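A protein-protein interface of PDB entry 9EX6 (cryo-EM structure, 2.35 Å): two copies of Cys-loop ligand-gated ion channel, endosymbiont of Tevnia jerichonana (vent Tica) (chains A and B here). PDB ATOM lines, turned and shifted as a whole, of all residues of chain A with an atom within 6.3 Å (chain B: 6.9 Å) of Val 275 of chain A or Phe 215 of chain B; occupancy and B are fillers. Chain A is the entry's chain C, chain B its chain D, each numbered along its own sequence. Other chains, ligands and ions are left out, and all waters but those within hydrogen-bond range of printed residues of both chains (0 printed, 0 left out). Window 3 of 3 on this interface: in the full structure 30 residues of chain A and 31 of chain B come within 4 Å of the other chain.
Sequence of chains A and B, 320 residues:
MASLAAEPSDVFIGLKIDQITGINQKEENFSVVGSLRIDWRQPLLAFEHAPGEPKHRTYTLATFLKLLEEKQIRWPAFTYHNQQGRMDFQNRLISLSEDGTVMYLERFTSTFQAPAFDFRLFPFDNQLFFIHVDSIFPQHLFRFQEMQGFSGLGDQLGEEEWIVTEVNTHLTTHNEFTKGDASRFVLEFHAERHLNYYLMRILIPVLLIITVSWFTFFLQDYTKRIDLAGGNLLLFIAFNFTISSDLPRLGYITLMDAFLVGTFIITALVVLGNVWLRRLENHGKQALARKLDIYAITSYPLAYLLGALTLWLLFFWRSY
Ile 226 of chain A touches Leu 228 of chain B (CG2 to CD2, 3.98 Å).
Leu 272 of chain A touches Thr 211 of chain B (CD1 to CG2, 3.9 Å).
Leu 272 of chain A touches Val 212 of chain B (CD2 to CG2, 3.99 Å).
Phe 215 of chain B touches Leu 272 of chain A.
Phe 215 of chain B touches Val 275 of chain A (O to CG1, 3.8 Å).
CG of Arg 278 of chain A touches CD2 of Leu 219 of chain B (3.7 Å).
Of the printed residues of chain B, Leu 272 of chain A touches Thr 211 (3.9 Å), Val 212 (3.99 Å) and Phe 215 (3.6 Å).
Of the printed residues of chain B, Val 275 of chain A touches Phe 215 (3.8 Å).
Of the printed residues of chain A, Thr 211 of chain B touches Leu 272.
Phe 215 of chain B touches just these residues of chain A: Leu 272 (3.6 Å) and Val 275 (3.8 Å).
Of the printed residues of chain A, Leu 219 of chain B touches Arg 278.
Of the printed residues of chain A, Leu 228 of chain B touches Ile 226 (3.98 Å).
The nearest printed residue of chain B that does not touch Leu 272 of chain A is Ser 213 of chain B (6.3 Å).
Hydrophobic or aromatic side chains of chain B that line the printed part of chain A: Val 212, Phe 215, Leu 219 and Leu 228.
Hydrophobic or aromatic side chains of chain A that line the printed part of chain B: Ile 226, Leu 272 and Val 275.
Along chain A the printed residues that touch a printed residue of chain B span positions 226 to 278.
Among the printed residues, no Asp or Glu carboxylate lies within 4 Å of a Lys or Arg side-chain nitrogen of the other chain.
No position is printed for both chains.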
ATOM      1  N   ILE A 226      12.340  11.884  36.638  1.00  0.00           N
ATOM      2  CA  ILE A 226      11.381  11.231  35.747  1.00  0.00           C
ATOM      3  C   ILE A 226      10.468  10.303  36.538  1.00  0.00           C
ATOM      4  O   ILE A 226       9.251  10.253  36.308  1.00  0.00           O
ATOM      5  CB  ILE A 226      12.118  10.482  34.622  1.00  0.00           C
ATOM      6  CG1 ILE A 226      12.901  11.467  33.759  1.00  0.00           C
ATOM      7  CG2 ILE A 226      11.133   9.712  33.771  1.00  0.00           C
ATOM      8  CD1 ILE A 226      13.906  10.817  32.845  1.00  0.00           C
ATOM      9  N   VAL A 270       5.480  18.075  32.150  1.00  0.00           N
ATOM     10  CA  VAL A 270       6.667  17.980  33.001  1.00  0.00           C
ATOM     11  C   VAL A 270       7.397  16.643  32.812  1.00  0.00           C
ATOM     12  O   VAL A 270       8.635  16.593  32.880  1.00  0.00           O
ATOM     13  CB  VAL A 270       6.273  18.220  34.474  1.00  0.00           C
ATOM     14  CG1 VAL A 270       7.479  18.065  35.383  1.00  0.00           C
ATOM     15  CG2 VAL A 270       5.690  19.614  34.641  1.00  0.00           C
ATOM     16  N   VAL A 271       6.657  15.562  32.557  1.00  0.00           N
ATOM     17  CA  VAL A 271       7.273  14.258  32.320  1.00  0.00           C
ATOM     18  C   VAL A 271       8.081  14.297  31.029  1.00  0.00           C
ATOM     19  O   VAL A 271       9.205  13.787  30.950  1.00  0.00           O
ATOM     20  CB  VAL A 271       6.205  13.152  32.255  1.00  0.00           C
ATOM     21  CG1 VAL A 271       6.899  11.818  32.197  1.00  0.00           C
ATOM     22  CG2 VAL A 271       5.325  13.199  33.486  1.00  0.00           C
ATOM     23  N   LEU A 272       7.520  14.916  30.003  1.00  0.00           N
ATOM     24  CA  LEU A 272       8.147  14.926  28.694  1.00  0.00           C
ATOM     25  C   LEU A 272       9.407  15.782  28.697  1.00  0.00           C
ATOM     26  O   LEU A 272      10.413  15.424  28.069  1.00  0.00           O
ATOM     27  CB  LEU A 272       7.132  15.433  27.681  1.00  0.00           C
ATOM     28  CG  LEU A 272       5.949  14.533  27.298  1.00  0.00           C
ATOM     29  CD1 LEU A 272       5.065  15.204  26.268  1.00  0.00           C
ATOM     30  CD2 LEU A 272       6.358  13.146  26.838  1.00  0.00           C
ATOM     31  N   GLY A 273       9.389  16.864  29.477  1.00  0.00           N
ATOM     32  CA  GLY A 273      10.537  17.751  29.535  1.00  0.00           C
ATOM     33  C   GLY A 273      11.745  17.118  30.194  1.00  0.00           C
ATOM     34  O   GLY A 273      12.881  17.286  29.738  1.00  0.00           O
ATOM     35  N   ASN A 274      11.513  16.389  31.292  1.00  0.00           N
ATOM     36  CA  ASN A 274      12.611  15.764  32.021  1.00  0.00           C
ATOM     37  C   ASN A 274      13.236  14.617  31.237  1.00  0.00           C
ATOM     38  O   ASN A 274      14.432  14.351  31.396  1.00  0.00           O
ATOM     39  CB  ASN A 274      12.128  15.289  33.390  1.00  0.00           C
ATOM     40  CG  ASN A 274      12.038  16.421  34.401  1.00  0.00           C
ATOM     41  OD1 ASN A 274      13.058  16.968  34.825  1.00  0.00           O
ATOM     42  ND2 ASN A 274      10.815  16.779  34.789  1.00  0.00           N
ATOM     43  N   VAL A 275      12.462  13.931  30.388  1.00  0.00           N
ATOM     44  CA  VAL A 275      13.074  12.951  29.487  1.00  0.00           C
ATOM     45  C   VAL A 275      14.020  13.641  28.510  1.00  0.00           C
ATOM     46  O   VAL A 275      15.108  13.134  28.211  1.00  0.00           O
ATOM     47  CB  VAL A 275      12.004  12.128  28.743  1.00  0.00           C
ATOM     48  CG1 VAL A 275      12.671  11.151  27.772  1.00  0.00           C
ATOM     49  CG2 VAL A 275      11.175  11.333  29.728  1.00  0.00           C
ATOM     50  N   TRP A 276      13.632  14.812  27.999  1.00  0.00           N
ATOM     51  CA  TRP A 276      14.510  15.484  27.043  1.00  0.00           C
ATOM     52  C   TRP A 276      15.778  16.023  27.707  1.00  0.00           C
ATOM     53  O   TRP A 276      16.849  15.999  27.086  1.00  0.00           O
ATOM     54  CB  TRP A 276      13.759  16.597  26.313  1.00  0.00           C
ATOM     55  CG  TRP A 276      14.500  17.111  25.099  1.00  0.00           C
ATOM     56  CD1 TRP A 276      15.243  18.250  25.003  1.00  0.00           C
ATOM     57  CD2 TRP A 276      14.572  16.484  23.818  1.00  0.00           C
ATOM     58  NE1 TRP A 276      15.793  18.356  23.746  1.00  0.00           N
ATOM     59  CE2 TRP A 276      15.378  17.292  22.991  1.00  0.00           C
ATOM     60  CE3 TRP A 276      14.061  15.303  23.301  1.00  0.00           C
ATOM     61  CZ2 TRP A 276      15.657  16.964  21.651  1.00  0.00           C
ATOM     62  CZ3 TRP A 276      14.303  14.998  21.958  1.00  0.00           C
ATOM     63  CH2 TRP A 276      15.115  15.815  21.163  1.00  0.00           C
ATOM     64  N   LEU A 277      15.696  16.475  28.964  1.00  0.00           N
ATOM     65  CA  LEU A 277      16.898  16.928  29.668  1.00  0.00           C
ATOM     66  C   LEU A 277      17.878  15.779  29.893  1.00  0.00           C
ATOM     67  O   LEU A 277      19.099  15.969  29.811  1.00  0.00           O
ATOM     68  CB  LEU A 277      16.524  17.597  30.995  1.00  0.00           C
ATOM     69  CG  LEU A 277      15.769  18.929  30.901  1.00  0.00           C
ATOM     70  CD1 LEU A 277      15.250  19.342  32.268  1.00  0.00           C
ATOM     71  CD2 LEU A 277      16.656  20.022  30.324  1.00  0.00           C
ATOM     72  N   ARG A 278      17.358  14.575  30.175  1.00  0.00           N
ATOM     73  CA  ARG A 278      18.211  13.394  30.293  1.00  0.00           C
ATOM     74  C   ARG A 278      18.881  13.050  28.965  1.00  0.00           C
ATOM     75  O   ARG A 278      20.026  12.588  28.953  1.00  0.00           O
ATOM     76  CB  ARG A 278      17.402  12.202  30.809  1.00  0.00           C
ATOM     77  CG  ARG A 278      18.186  10.891  31.035  1.00  0.00           C
ATOM     78  CD  ARG A 278      19.437  10.999  31.903  1.00  0.00           C
ATOM     79  NE  ARG A 278      20.032   9.684  32.137  1.00  0.00           N
ATOM     80  CZ  ARG A 278      21.218   9.459  32.684  1.00  0.00           C
ATOM     81  NH1 ARG A 278      22.036  10.445  32.987  1.00  0.00           N
ATOM     82  NH2 ARG A 278      21.624   8.202  32.852  1.00  0.00           N
ATOM     83  N   ARG A 279      18.190  13.275  27.844  1.00  0.00           N
ATOM     84  CA  ARG A 279      18.788  12.996  26.542  1.00  0.00           C
ATOM     85  C   ARG A 279      19.951  13.940  26.274  1.00  0.00           C
ATOM     86  O   ARG A 279      20.994  13.518  25.764  1.00  0.00           O
ATOM     87  CB  ARG A 279      17.744  13.120  25.432  1.00  0.00           C
ATOM     88  CG  ARG A 279      18.230  12.633  24.074  1.00  0.00           C
ATOM     89  CD  ARG A 279      17.281  13.002  22.935  1.00  0.00           C
ATOM     90  NE  ARG A 279      17.589  12.248  21.725  1.00  0.00           N
ATOM     91  CZ  ARG A 279      18.179  12.732  20.637  1.00  0.00           C
ATOM     92  NH1 ARG A 279      18.483  14.016  20.523  1.00  0.00           N
ATOM     93  NH2 ARG A 279      18.469  11.908  19.637  1.00  0.00           N
ATOM     94  N   LEU A 280      19.784  15.222  26.616  1.00  0.00           N
ATOM     95  CA  LEU A 280      20.862  16.190  26.439  1.00  0.00           C
ATOM     96  C   LEU A 280      22.076  15.825  27.290  1.00  0.00           C
ATOM     97  O   LEU A 280      23.220  15.955  26.840  1.00  0.00           O
ATOM     98  CB  LEU A 280      20.366  17.601  26.776  1.00  0.00           C
ATOM     99  CG  LEU A 280      19.266  18.186  25.887  1.00  0.00           C
ATOM    100  CD1 LEU A 280      18.772  19.492  26.441  1.00  0.00           C
ATOM    101  CD2 LEU A 280      19.918  18.470  24.535  1.00  0.00           C
ATOM    102  N   ILE B 210      -0.262   8.474  24.845  1.00  0.00           N
ATOM    103  CA  ILE B 210       0.402   7.878  23.697  1.00  0.00           C
ATOM    104  C   ILE B 210       1.766   8.520  23.474  1.00  0.00           C
ATOM    105  O   ILE B 210       2.741   7.843  23.116  1.00  0.00           O
ATOM    106  CB  ILE B 210      -0.519   7.980  22.465  1.00  0.00           C
ATOM    107  CG1 ILE B 210      -1.590   6.890  22.531  1.00  0.00           C
ATOM    108  CG2 ILE B 210       0.263   7.782  21.184  1.00  0.00           C
ATOM    109  CD1 ILE B 210      -2.731   7.068  21.571  1.00  0.00           C
ATOM    110  N   THR B 211       1.874   9.821  23.749  1.00  0.00           N
ATOM    111  CA  THR B 211       3.137  10.518  23.529  1.00  0.00           C
ATOM    112  C   THR B 211       4.194  10.110  24.559  1.00  0.00           C
ATOM    113  O   THR B 211       5.380   9.987  24.221  1.00  0.00           O
ATOM    114  CB  THR B 211       2.906  12.029  23.526  1.00  0.00           C
ATOM    115  OG1 THR B 211       2.066  12.382  22.424  1.00  0.00           O
ATOM    116  CG2 THR B 211       4.232  12.746  23.320  1.00  0.00           C
ATOM    117  N   VAL B 212       3.773   9.873  25.800  1.00  0.00           N
ATOM    118  CA  VAL B 212       4.702   9.459  26.845  1.00  0.00           C
ATOM    119  C   VAL B 212       5.307   8.106  26.496  1.00  0.00           C
ATOM    120  O   VAL B 212       6.508   7.877  26.691  1.00  0.00           O
ATOM    121  CB  VAL B 212       4.003   9.425  28.216  1.00  0.00           C
ATOM    122  CG1 VAL B 212       4.910   8.779  29.250  1.00  0.00           C
ATOM    123  CG2 VAL B 212       3.668  10.834  28.657  1.00  0.00           C
ATOM    124  N   SER B 213       4.489   7.196  25.956  1.00  0.00           N
ATOM    125  CA  SER B 213       4.999   5.891  25.544  1.00  0.00           C
ATOM    126  C   SER B 213       6.020   5.997  24.413  1.00  0.00           C
ATOM    127  O   SER B 213       6.976   5.214  24.386  1.00  0.00           O
ATOM    128  CB  SER B 213       3.848   4.979  25.132  1.00  0.00           C
ATOM    129  OG  SER B 213       3.326   4.271  26.243  1.00  0.00           O
ATOM    130  N   TRP B 214       5.840   6.938  23.480  1.00  0.00           N
ATOM    131  CA  TRP B 214       6.822   7.105  22.406  1.00  0.00           C
ATOM    132  C   TRP B 214       8.155   7.623  22.941  1.00  0.00           C
ATOM    133  O   TRP B 214       9.221   7.283  22.414  1.00  0.00           O
ATOM    134  CB  TRP B 214       6.267   8.053  21.332  1.00  0.00           C
ATOM    135  CG  TRP B 214       7.073   8.072  20.045  1.00  0.00           C
ATOM    136  CD1 TRP B 214       7.541   6.995  19.341  1.00  0.00           C
ATOM    137  CD2 TRP B 214       7.485   9.232  19.311  1.00  0.00           C
ATOM    138  NE1 TRP B 214       8.225   7.415  18.226  1.00  0.00           N
ATOM    139  CE2 TRP B 214       8.205   8.783  18.182  1.00  0.00           C
ATOM    140  CE3 TRP B 214       7.297  10.604  19.486  1.00  0.00           C
ATOM    141  CZ2 TRP B 214       8.760   9.662  17.247  1.00  0.00           C
ATOM    142  CZ3 TRP B 214       7.890  11.473  18.588  1.00  0.00           C
ATOM    143  CH2 TRP B 214       8.580  10.999  17.461  1.00  0.00           C
ATOM    144  N   PHE B 215       8.114   8.513  23.941  1.00  0.00           N
ATOM    145  CA  PHE B 215       9.321   9.185  24.431  1.00  0.00           C
ATOM    146  C   PHE B 215      10.284   8.214  25.111  1.00  0.00           C
ATOM    147  O   PHE B 215      11.460   8.549  25.292  1.00  0.00           O
ATOM    148  CB  PHE B 215       8.961  10.329  25.389  1.00  0.00           C
ATOM    149  CG  PHE B 215       8.983  11.713  24.756  1.00  0.00           C
ATOM    150  CD1 PHE B 215       8.183  12.004  23.663  1.00  0.00           C
ATOM    151  CD2 PHE B 215       9.744  12.742  25.311  1.00  0.00           C
ATOM    152  CE1 PHE B 215       8.170  13.271  23.092  1.00  0.00           C
ATOM    153  CE2 PHE B 215       9.733  14.018  24.746  1.00  0.00           C
ATOM    154  CZ  PHE B 215       8.938  14.282  23.637  1.00  0.00           C
ATOM    155  N   THR B 216       9.810   7.014  25.463  1.00  0.00           N
ATOM    156  CA  THR B 216      10.659   6.000  26.082  1.00  0.00           C
ATOM    157  C   THR B 216      11.824   5.580  25.185  1.00  0.00           C
ATOM    158  O   THR B 216      12.903   5.263  25.699  1.00  0.00           O
ATOM    159  CB  THR B 216       9.795   4.794  26.472  1.00  0.00           C
ATOM    160  OG1 THR B 216       8.980   5.123  27.605  1.00  0.00           O
ATOM    161  CG2 THR B 216      10.642   3.575  26.804  1.00  0.00           C
ATOM    162  N   PHE B 217      11.643   5.616  23.865  1.00  0.00           N
ATOM    163  CA  PHE B 217      12.687   5.230  22.919  1.00  0.00           C
ATOM    164  C   PHE B 217      13.818   6.252  22.838  1.00  0.00           C
ATOM    165  O   PHE B 217      14.799   5.995  22.134  1.00  0.00           O
ATOM    166  CB  PHE B 217      12.073   4.989  21.538  1.00  0.00           C
ATOM    167  CG  PHE B 217      11.101   3.829  21.490  1.00  0.00           C
ATOM    168  CD1 PHE B 217      11.560   2.520  21.510  1.00  0.00           C
ATOM    169  CD2 PHE B 217       9.735   4.050  21.411  1.00  0.00           C
ATOM    170  CE1 PHE B 217      10.673   1.455  21.459  1.00  0.00           C
ATOM    171  CE2 PHE B 217       8.838   2.988  21.364  1.00  0.00           C
ATOM    172  CZ  PHE B 217       9.308   1.691  21.389  1.00  0.00           C
ATOM    173  N   PHE B 218      13.727   7.376  23.559  1.00  0.00           N
ATOM    174  CA  PHE B 218      14.742   8.425  23.507  1.00  0.00           C
ATOM    175  C   PHE B 218      15.861   8.195  24.523  1.00  0.00           C
ATOM    176  O   PHE B 218      16.883   8.886  24.458  1.00  0.00           O
ATOM    177  CB  PHE B 218      14.128   9.823  23.748  1.00  0.00           C
ATOM    178  CG  PHE B 218      13.101  10.279  22.710  1.00  0.00           C
ATOM    179  CD1 PHE B 218      12.866   9.572  21.539  1.00  0.00           C
ATOM    180  CD2 PHE B 218      12.362  11.436  22.935  1.00  0.00           C
ATOM    181  CE1 PHE B 218      11.920  10.023  20.616  1.00  0.00           C
ATOM    182  CE2 PHE B 218      11.441  11.899  22.016  1.00  0.00           C
ATOM    183  CZ  PHE B 218      11.205  11.191  20.864  1.00  0.00           C
ATOM    184  N   LEU B 219      15.694   7.242  25.446  1.00  0.00           N
ATOM    185  CA  LEU B 219      16.617   6.969  26.544  1.00  0.00           C
ATOM    186  C   LEU B 219      17.533   5.792  26.212  1.00  0.00           C
ATOM    187  O   LEU B 219      17.247   4.986  25.323  1.00  0.00           O
ATOM    188  CB  LEU B 219      15.848   6.680  27.839  1.00  0.00           C
ATOM    189  CG  LEU B 219      14.962   7.797  28.404  1.00  0.00           C
ATOM    190  CD1 LEU B 219      13.865   7.206  29.296  1.00  0.00           C
ATOM    191  CD2 LEU B 219      15.735   8.913  29.077  1.00  0.00           C
ATOM    192  N   LEU B 228       9.519   2.309  33.041  1.00  0.00           N
ATOM    193  CA  LEU B 228       8.710   3.436  32.594  1.00  0.00           C
ATOM    194  C   LEU B 228       7.555   2.984  31.704  1.00  0.00           C
ATOM    195  O   LEU B 228       6.431   3.494  31.820  1.00  0.00           O
ATOM    196  CB  LEU B 228       9.593   4.464  31.882  1.00  0.00           C
ATOM    197  CG  LEU B 228      10.636   5.166  32.762  1.00  0.00           C
ATOM    198  CD1 LEU B 228      11.512   6.118  31.963  1.00  0.00           C
ATOM    199  CD2 LEU B 228       9.975   5.907  33.910  1.00  0.00           C
ATOM    200  N   TYR B 300       6.529   3.281  15.184  1.00  0.00           N
ATOM    201  CA  TYR B 300       5.481   3.502  16.185  1.00  0.00           C
ATOM    202  C   TYR B 300       4.399   4.475  15.717  1.00  0.00           C
ATOM    203  O   TYR B 300       3.208   4.132  15.819  1.00  0.00           O
ATOM    204  CB  TYR B 300       6.129   3.958  17.507  1.00  0.00           C
ATOM    205  CG  TYR B 300       5.181   4.243  18.666  1.00  0.00           C
ATOM    206  CD1 TYR B 300       4.640   5.505  18.855  1.00  0.00           C
ATOM    207  CD2 TYR B 300       4.899   3.268  19.613  1.00  0.00           C
ATOM    208  CE1 TYR B 300       3.802   5.774  19.925  1.00  0.00           C
ATOM    209  CE2 TYR B 300       4.059   3.529  20.688  1.00  0.00           C
ATOM    210  CZ  TYR B 300       3.509   4.782  20.837  1.00  0.00           C
ATOM    211  OH  TYR B 300       2.664   5.042  21.897  1.00  0.00           O
